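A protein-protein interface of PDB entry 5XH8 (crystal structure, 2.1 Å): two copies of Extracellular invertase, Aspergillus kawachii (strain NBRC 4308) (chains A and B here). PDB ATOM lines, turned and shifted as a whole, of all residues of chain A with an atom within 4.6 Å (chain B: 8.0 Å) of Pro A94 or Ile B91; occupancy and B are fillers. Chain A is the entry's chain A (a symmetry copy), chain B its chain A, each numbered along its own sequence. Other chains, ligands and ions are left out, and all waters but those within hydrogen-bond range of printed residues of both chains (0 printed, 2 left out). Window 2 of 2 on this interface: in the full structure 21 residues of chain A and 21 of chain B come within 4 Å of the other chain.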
ATOM      1  N   GLY A  89     -17.084   6.009  17.839  1.00  0.00           N
ATOM      2  CA  GLY A  89     -16.298   5.504  16.709  1.00  0.00           C
ATOM      3  C   GLY A  89     -17.003   5.656  15.364  1.00  0.00           C
ATOM      4  O   GLY A  89     -16.471   5.240  14.374  1.00  0.00           O
ATOM      5  N   GLY A  90     -18.187   6.263  15.323  1.00  0.00           N
ATOM      6  CA  GLY A  90     -18.847   6.591  14.044  1.00  0.00           C
ATOM      7  C   GLY A  90     -18.266   7.837  13.401  1.00  0.00           C
ATOM      8  O   GLY A  90     -17.365   8.489  13.945  1.00  0.00           O
ATOM      9  N   ILE A  91     -18.854   8.209  12.276  1.00  0.00           N
ATOM     10  CA  ILE A  91     -18.484   9.404  11.558  1.00  0.00           C
ATOM     11  C   ILE A  91     -18.783  10.673  12.401  1.00  0.00           C
ATOM     12  O   ILE A  91     -17.975  11.636  12.429  1.00  0.00           O
ATOM     13  CB  ILE A  91     -19.224   9.468  10.209  1.00  0.00           C
ATOM     14  CG1 ILE A  91     -18.828   8.275   9.296  1.00  0.00           C
ATOM     15  CG2 ILE A  91     -19.004  10.802   9.518  1.00  0.00           C
ATOM     16  CD1 ILE A  91     -17.444   8.349   8.704  1.00  0.00           C
ATOM     17  N   ASN A  92     -19.933  10.680  13.064  1.00  0.00           N
ATOM     18  CA  ASN A  92     -20.363  11.876  13.828  1.00  0.00           C
ATOM     19  C   ASN A  92     -19.810  11.907  15.231  1.00  0.00           C
ATOM     20  O   ASN A  92     -19.709  12.993  15.828  1.00  0.00           O
ATOM     21  CB  ASN A  92     -21.869  11.964  13.917  1.00  0.00           C
ATOM     22  CG  ASN A  92     -22.559  11.979  12.555  1.00  0.00           C
ATOM     23  OD1 ASN A  92     -21.955  12.270  11.503  1.00  0.00           O
ATOM     24  ND2 ASN A  92     -23.858  11.686  12.583  1.00  0.00           N
ATOM     25  N   ASP A  93     -19.486  10.728  15.770  1.00  0.00           N
ATOM     26  CA  ASP A  93     -19.052  10.586  17.170  1.00  0.00           C
ATOM     27  C   ASP A  93     -17.743   9.782  17.278  1.00  0.00           C
ATOM     28  O   ASP A  93     -17.681   8.791  18.003  1.00  0.00           O
ATOM     29  CB  ASP A  93     -20.165   9.958  18.026  1.00  0.00           C
ATOM     30  CG  ASP A  93     -20.724   8.661  17.450  1.00  0.00           C
ATOM     31  OD1 ASP A  93     -20.178   8.119  16.468  1.00  0.00           O
ATOM     32  OD2 ASP A  93     -21.738   8.187  18.004  1.00  0.00           O
ATOM     33  N   PRO A  94     -16.695  10.200  16.542  1.00  0.00           N
ATOM     34  CA  PRO A  94     -15.462   9.397  16.539  1.00  0.00           C
ATOM     35  C   PRO A  94     -14.785   9.346  17.912  1.00  0.00           C
ATOM     36  O   PRO A  94     -14.097   8.379  18.199  1.00  0.00           O
ATOM     37  CB  PRO A  94     -14.571  10.123  15.500  1.00  0.00           C
ATOM     38  CG  PRO A  94     -15.060  11.566  15.550  1.00  0.00           C
ATOM     39  CD  PRO A  94     -16.551  11.443  15.768  1.00  0.00           C
ATOM     40  N   VAL A  95     -15.015  10.348  18.779  1.00  0.00           N
ATOM     41  CA  VAL A  95     -14.315  10.426  20.061  1.00  0.00           C
ATOM     42  C   VAL A  95     -15.185   9.916  21.213  1.00  0.00           C
ATOM     43  O   VAL A  95     -14.699   9.156  22.037  1.00  0.00           O
ATOM     44  CB  VAL A  95     -13.785  11.861  20.301  1.00  0.00           C
ATOM     45  CG1 VAL A  95     -13.268  12.047  21.718  1.00  0.00           C
ATOM     46  CG2 VAL A  95     -12.690  12.160  19.285  1.00  0.00           C
ATOM     47  N   ALA A  96     -16.453  10.319  21.291  1.00  0.00           N
ATOM     48  CA  ALA A  96     -17.278   9.919  22.428  1.00  0.00           C
ATOM     49  C   ALA A  96     -18.765   9.983  22.130  1.00  0.00           C
ATOM     50  O   ALA A  96     -19.209  10.712  21.210  1.00  0.00           O
ATOM     51  CB  ALA A  96     -16.944  10.785  23.650  1.00  0.00           C
ATOM     52  N   VAL A 118     -19.696  13.314  20.009  1.00  0.00           N
ATOM     53  CA  VAL A 118     -18.486  14.063  20.338  1.00  0.00           C
ATOM     54  C   VAL A 118     -17.326  13.758  19.353  1.00  0.00           C
ATOM     55  O   VAL A 118     -16.968  12.590  19.100  1.00  0.00           O
ATOM     56  CB  VAL A 118     -18.059  13.811  21.782  1.00  0.00           C
ATOM     57  CG1 VAL A 118     -16.738  14.505  22.129  1.00  0.00           C
ATOM     58  CG2 VAL A 118     -19.157  14.245  22.751  1.00  0.00           C
ATOM     59  N   SER A 119     -16.768  14.830  18.787  1.00  0.00           N
ATOM     60  CA  SER A 119     -15.673  14.755  17.812  1.00  0.00           C
ATOM     61  C   SER A 119     -14.326  15.335  18.273  1.00  0.00           C
ATOM     62  O   SER A 119     -13.301  15.098  17.615  1.00  0.00           O
ATOM     63  CB  SER A 119     -16.095  15.449  16.533  1.00  0.00           C
ATOM     64  OG  SER A 119     -17.240  14.844  15.981  1.00  0.00           O
ATOM     65  N   TYR A 120     -14.318  16.088  19.375  1.00  0.00           N
ATOM     66  CA  TYR A 120     -13.102  16.753  19.892  1.00  0.00           C
ATOM     67  C   TYR A 120     -13.160  16.835  21.406  1.00  0.00           C
ATOM     68  O   TYR A 120     -14.211  17.154  21.970  1.00  0.00           O
ATOM     69  CB  TYR A 120     -12.939  18.189  19.350  1.00  0.00           C
ATOM     70  CG  TYR A 120     -12.750  18.209  17.867  1.00  0.00           C
ATOM     71  CD1 TYR A 120     -11.489  17.989  17.294  1.00  0.00           C
ATOM     72  CD2 TYR A 120     -13.837  18.393  17.018  1.00  0.00           C
ATOM     73  CE1 TYR A 120     -11.335  17.942  15.916  1.00  0.00           C
ATOM     74  CE2 TYR A 120     -13.693  18.324  15.634  1.00  0.00           C
ATOM     75  CZ  TYR A 120     -12.451  18.103  15.088  1.00  0.00           C
ATOM     76  OH  TYR A 120     -12.316  18.060  13.722  1.00  0.00           O
ATOM     77  N   PRO B  88      -7.811  13.170   2.520  1.00  0.00           N
ATOM     78  CA  PRO B  88      -8.941  12.791   3.375  1.00  0.00           C
ATOM     79  C   PRO B  88      -8.535  11.886   4.533  1.00  0.00           C
ATOM     80  O   PRO B  88      -7.390  11.451   4.590  1.00  0.00           O
ATOM     81  CB  PRO B  88      -9.866  12.038   2.408  1.00  0.00           C
ATOM     82  CG  PRO B  88      -8.947  11.475   1.376  1.00  0.00           C
ATOM     83  CD  PRO B  88      -7.843  12.480   1.215  1.00  0.00           C
ATOM     84  N   GLY B  89      -9.473  11.591   5.426  1.00  0.00           N
ATOM     85  CA  GLY B  89      -9.220  10.708   6.569  1.00  0.00           C
ATOM     86  C   GLY B  89      -9.179  11.443   7.905  1.00  0.00           C
ATOM     87  O   GLY B  89      -8.939  10.827   8.906  1.00  0.00           O
ATOM     88  N   GLY B  90      -9.428  12.751   7.929  1.00  0.00           N
ATOM     89  CA  GLY B  90      -9.568  13.491   9.198  1.00  0.00           C
ATOM     90  C   GLY B  90     -10.933  13.292   9.831  1.00  0.00           C
ATOM     91  O   GLY B  90     -11.807  12.605   9.288  1.00  0.00           O
ATOM     92  N   ILE B  91     -11.134  13.975  10.947  1.00  0.00           N
ATOM     93  CA  ILE B  91     -12.391  13.965  11.653  1.00  0.00           C
ATOM     94  C   ILE B  91     -13.517  14.600  10.793  1.00  0.00           C
ATOM     95  O   ILE B  91     -14.668  14.095  10.760  1.00  0.00           O
ATOM     96  CB  ILE B  91     -12.256  14.709  12.996  1.00  0.00           C
ATOM     97  CG1 ILE B  91     -11.232  14.003  13.926  1.00  0.00           C
ATOM     98  CG2 ILE B  91     -13.604  14.882  13.672  1.00  0.00           C
ATOM     99  CD1 ILE B  91     -11.697  12.704  14.529  1.00  0.00           C
ATOM    100  N   ASN B  92     -13.194  15.697  10.120  1.00  0.00           N
ATOM    101  CA  ASN B  92     -14.213  16.438   9.338  1.00  0.00           C
ATOM    102  C   ASN B  92     -14.386  15.899   7.940  1.00  0.00           C
ATOM    103  O   ASN B  92     -15.451  16.101   7.330  1.00  0.00           O
ATOM    104  CB  ASN B  92     -13.872  17.906   9.234  1.00  0.00           C
ATOM    105  CG  ASN B  92     -13.704  18.589  10.590  1.00  0.00           C
ATOM    106  OD1 ASN B  92     -14.163  18.103  11.644  1.00  0.00           O
ATOM    107  ND2 ASN B  92     -13.057  19.752  10.553  1.00  0.00           N
ATOM    108  N   ASP B  93     -13.341  15.250   7.418  1.00  0.00           N
ATOM    109  CA  ASP B  93     -13.316  14.776   6.023  1.00  0.00           C
ATOM    110  C   ASP B  93     -12.912  13.293   5.937  1.00  0.00           C
ATOM    111  O   ASP B  93     -11.972  12.945   5.224  1.00  0.00           O
ATOM    112  CB  ASP B  93     -12.391  15.657   5.165  1.00  0.00           C
ATOM    113  CG  ASP B  93     -10.995  15.835   5.751  1.00  0.00           C
ATOM    114  OD1 ASP B  93     -10.638  15.170   6.744  1.00  0.00           O
ATOM    115  OD2 ASP B  93     -10.249  16.668   5.194  1.00  0.00           O
ATOM    116  N   PRO B  94     -13.615  12.413   6.677  1.00  0.00           N
ATOM    117  CA  PRO B  94     -13.193  11.005   6.700  1.00  0.00           C
ATOM    118  C   PRO B  94     -13.322  10.324   5.334  1.00  0.00           C
ATOM    119  O   PRO B  94     -12.585   9.388   5.065  1.00  0.00           O
ATOM    120  CB  PRO B  94     -14.150  10.367   7.738  1.00  0.00           C
ATOM    121  CG  PRO B  94     -15.395  11.241   7.667  1.00  0.00           C
ATOM    122  CD  PRO B  94     -14.855  12.635   7.437  1.00  0.00           C
ATOM    123  N   VAL B  95     -14.211  10.817   4.453  1.00  0.00           N
ATOM    124  CA  VAL B  95     -14.471  10.152   3.177  1.00  0.00           C
ATOM    125  C   VAL B  95     -13.727  10.830   2.022  1.00  0.00           C
ATOM    126  O   VAL B  95     -13.127  10.140   1.213  1.00  0.00           O
ATOM    127  CB  VAL B  95     -15.995  10.045   2.924  1.00  0.00           C
ATOM    128  CG1 VAL B  95     -16.307   9.585   1.510  1.00  0.00           C
ATOM    129  CG2 VAL B  95     -16.600   9.091   3.947  1.00  0.00           C
ATOM    130  N   TYR B 115     -12.179  24.652   2.406  1.00  0.00           N
ATOM    131  CA  TYR B 115     -12.453  23.561   1.469  1.00  0.00           C
ATOM    132  C   TYR B 115     -13.624  22.708   1.897  1.00  0.00           C
ATOM    133  O   TYR B 115     -14.033  22.711   3.085  1.00  0.00           O
ATOM    134  CB  TYR B 115     -11.206  22.682   1.312  1.00  0.00           C
ATOM    135  CG  TYR B 115     -10.904  21.748   2.486  1.00  0.00           C
ATOM    136  CD1 TYR B 115     -10.250  22.216   3.624  1.00  0.00           C
ATOM    137  CD2 TYR B 115     -11.268  20.410   2.449  1.00  0.00           C
ATOM    138  CE1 TYR B 115      -9.979  21.372   4.690  1.00  0.00           C
ATOM    139  CE2 TYR B 115     -11.016  19.565   3.522  1.00  0.00           C
ATOM    140  CZ  TYR B 115     -10.367  20.047   4.641  1.00  0.00           C
ATOM    141  OH  TYR B 115     -10.085  19.203   5.683  1.00  0.00           O
ATOM    142  N   SER B 117     -15.074  19.516   3.048  1.00  0.00           N
ATOM    143  CA  SER B 117     -14.759  18.301   3.786  1.00  0.00           C
ATOM    144  C   SER B 117     -15.960  17.337   3.672  1.00  0.00           C
ATOM    145  O   SER B 117     -17.077  17.710   4.012  1.00  0.00           O
ATOM    146  CB  SER B 117     -14.434  18.661   5.236  1.00  0.00           C
ATOM    147  OG  SER B 117     -15.298  19.656   5.764  1.00  0.00           O
ATOM    148  N   VAL B 118     -15.726  16.129   3.146  1.00  0.00           N
ATOM    149  CA  VAL B 118     -16.783  15.175   2.819  1.00  0.00           C
ATOM    150  C   VAL B 118     -16.826  13.988   3.818  1.00  0.00           C
ATOM    151  O   VAL B 118     -15.808  13.319   4.089  1.00  0.00           O
ATOM    152  CB  VAL B 118     -16.648  14.677   1.382  1.00  0.00           C
ATOM    153  CG1 VAL B 118     -17.684  13.602   1.039  1.00  0.00           C
ATOM    154  CG2 VAL B 118     -16.747  15.842   0.399  1.00  0.00           C
ATOM    155  N   SER B 119     -18.016  13.762   4.377  1.00  0.00           N
ATOM    156  CA  SER B 119     -18.262  12.702   5.362  1.00  0.00           C
ATOM    157  C   SER B 119     -19.195  11.567   4.906  1.00  0.00           C
ATOM    158  O   SER B 119     -19.261  10.526   5.576  1.00  0.00           O
ATOM    159  CB  SER B 119     -18.820  13.317   6.629  1.00  0.00           C
ATOM    160  OG  SER B 119     -17.922  14.252   7.177  1.00  0.00           O
ATOM    161  N   THR B 135     -19.356  19.678   4.341  1.00  0.00           N
ATOM    162  CA  THR B 135     -19.127  20.788   5.257  1.00  0.00           C
ATOM    163  C   THR B 135     -17.946  21.584   4.715  1.00  0.00           C
ATOM    164  O   THR B 135     -17.251  21.144   3.789  1.00  0.00           O
ATOM    165  CB  THR B 135     -18.850  20.300   6.679  1.00  0.00           C
ATOM    166  OG1 THR B 135     -17.704  19.450   6.696  1.00  0.00           O
ATOM    167  CG2 THR B 135     -20.033  19.502   7.230  1.00  0.00           C
ATOM    168  N   SER B 137     -14.394  23.387   5.851  1.00  0.00           N
ATOM    169  CA  SER B 137     -13.393  23.322   6.911  1.00  0.00           C
ATOM    170  C   SER B 137     -12.190  24.151   6.554  1.00  0.00           C
ATOM    171  O   SER B 137     -11.986  24.497   5.374  1.00  0.00           O
ATOM    172  CB  SER B 137     -12.977  21.869   7.166  1.00  0.00           C
ATOM    173  OG  SER B 137     -14.057  21.136   7.731  1.00  0.00           O
ATOM    174  N   LYS B 150      -4.802  20.665   8.729  1.00  0.00           N
ATOM    175  CA  LYS B 150      -6.190  20.899   9.103  1.00  0.00           C
ATOM    176  C   LYS B 150      -6.256  21.506  10.489  1.00  0.00           C
ATOM    177  O   LYS B 150      -5.582  21.036  11.389  1.00  0.00           O
ATOM    178  CB  LYS B 150      -6.968  19.599   9.072  1.00  0.00           C
ATOM    179  CG  LYS B 150      -7.007  18.980   7.674  1.00  0.00           C
ATOM    180  CD  LYS B 150      -7.441  17.529   7.745  1.00  0.00           C
ATOM    181  CE  LYS B 150      -7.282  16.832   6.411  1.00  0.00           C
ATOM    182  NZ  LYS B 150      -7.775  15.434   6.503  1.00  0.00           N
ATOM    183  N   LEU B 151      -7.045  22.558  10.658  1.00  0.00           N
ATOM    184  CA  LEU B 151      -7.294  23.068  12.000  1.00  0.00           C
ATOM    185  C   LEU B 151      -8.006  21.975  12.800  1.00  0.00           C
ATOM    186  O   LEU B 151      -8.892  21.274  12.269  1.00  0.00           O
ATOM    187  CB  LEU B 151      -8.165  24.339  11.978  1.00  0.00           C
ATOM    188  CG  LEU B 151      -7.610  25.603  11.331  1.00  0.00           C
ATOM    189  CD1 LEU B 151      -8.463  26.778  11.782  1.00  0.00           C
ATOM    190  CD2 LEU B 151      -6.134  25.845  11.664  1.00  0.00           C
ATOM    191  N   ASP B 152      -7.601  21.837  14.060  1.00  0.00           N
ATOM    192  CA  ASP B 152      -8.080  20.799  14.939  1.00  0.00           C
ATOM    193  C   ASP B 152      -9.384  21.234  15.579  1.00  0.00           C
ATOM    194  O   ASP B 152      -9.471  21.508  16.763  1.00  0.00           O
ATOM    195  CB  ASP B 152      -7.001  20.454  15.972  1.00  0.00           C
ATOM    196  CG  ASP B 152      -7.266  19.140  16.683  1.00  0.00           C
ATOM    197  OD1 ASP B 152      -8.111  18.349  16.246  1.00  0.00           O
ATOM    198  OD2 ASP B 152      -6.618  18.883  17.703  1.00  0.00           O
ATOM    199  N   GLN B 153     -10.417  21.258  14.756  1.00  0.00           N
ATOM    200  CA  GLN B 153     -11.726  21.676  15.158  1.00  0.00           C
ATOM    201  C   GLN B 153     -12.699  21.279  14.053  1.00  0.00           C
ATOM    202  O   GLN B 153     -12.288  20.874  12.967  1.00  0.00           O
ATOM    203  CB  GLN B 153     -11.775  23.184  15.392  1.00  0.00           C
ATOM    204  CG  GLN B 153     -11.437  23.991  14.146  1.00  0.00           C
ATOM    205  CD  GLN B 153     -12.055  25.345  14.181  1.00  0.00           C
ATOM    206  OE1 GLN B 153     -11.554  26.218  14.849  1.00  0.00           O
ATOM    207  NE2 GLN B 153     -13.176  25.513  13.509  1.00  0.00           N
ATOM    208  N   GLY B 154     -13.985  21.430  14.344  1.00  0.00           N
ATOM    209  CA  GLY B 154     -15.029  21.123  13.389  1.00  0.00           C
ATOM    210  C   GLY B 154     -15.087  22.100  12.230  1.00  0.00           C
ATOM    211  O   GLY B 154     -14.363  23.108  12.216  1.00  0.00           O
ATOM    212  N   PRO B 155     -15.950  21.801  11.240  1.00  0.00           N
ATOM    213  CA  PRO B 155     -16.147  22.703  10.115  1.00  0.00           C
ATOM    214  C   PRO B 155     -16.603  24.109  10.565  1.00  0.00           C
ATOM    215  O   PRO B 155     -17.349  24.259  11.550  1.00  0.00           O
ATOM    216  CB  PRO B 155     -17.252  22.036   9.299  1.00  0.00           C
ATOM    217  CG  PRO B 155     -17.932  21.083  10.245  1.00  0.00           C
ATOM    218  CD  PRO B 155     -16.876  20.653  11.219  1.00  0.00           C
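OG of Ser B119 sits at hydrogen-bond distance from O of Asn B92. OG of Ser B137 sits at hydrogen-bond distance from ND2 of Asn B92 (3.3 Å). ND2 of Asn B92 lies within hydrogen-bond range of O of Gln B153 (2.8 Å). The side-chain hydroxyl (OG) of Ser A119 lies within hydrogen-bond range of the backbone carbonyl oxygen (O) of Asn A92 (3.1 Å).
Of the 11 printed residues of chain A, 4 touch a printed residue of chain B. Hydrophobic or aromatic side chains of chain A that line the printed part of chain B: Ile A91, Pro A94 and Tyr A120. Along chain A the printed residues that touch a printed residue of chain B span positions 91 to 120. Printed residues of chain B that touch a printed residue of chain A: Ile B91, Asn B92, Pro B94, Ser B119, Asp B152, Gln B153 and Gly B154. Among the printed residues, 9 pairs touch across the chains. Among the printed residues, no Asp or Glu carboxylate lies within 4 Å of a Lys or Arg side-chain nitrogen of the other chain.
Ile A91 touches Pro B94, and with the chains exchanged Pro A94 touches Ile B91. Ile A91 touches Ser B119, and with the chains exchanged Ser A119 touches Ile B91. 9 positions are printed for both chains. Of the 9 pairs that touch across the chains among the printed residues, 4 have their exchanged pair printed and touching as well.
OD1 of Asn B92 lies within hydrogen-bond range of OH of Tyr A120 (2.8 Å). The backbone carbonyl oxygen of Gln B153 is in hydrogen-bond range of the side-chain hydroxyl of Tyr A120 (2.9 Å).
Of the printed residues of chain B, Ile A91 touches Pro B94 and Ser B119. Printed residues of chain B within 4 Å of Tyr A120: Ile B91, Asn B92, Asp B152, Gln B153 and Gly B154. Ile B91 touches just these residues of chain A: Pro A94, Ser A119 and Tyr A120. The nearest residue of chain A that does not touch Ile B91 is Ile A91 (4.4 Å). The nearest printed residue of chain A that does not touch Gly B154 is Ser A119 (6.6 Å).
Ile A91 touches Pro B94 (CD1 to CG, 3.7 Å). Ile A91 touches Ser B119. Pro A94 touches Ile B91 (CG to CD1, 3.7 Å). CB of Ser A119 touches CG2 of Ile B91, 3.8 Å away. Ile B91 touches Tyr A120. Asp B152 touches Tyr A120. CE2 of Tyr A120 touches N of Gly B154 (3.4 Å).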
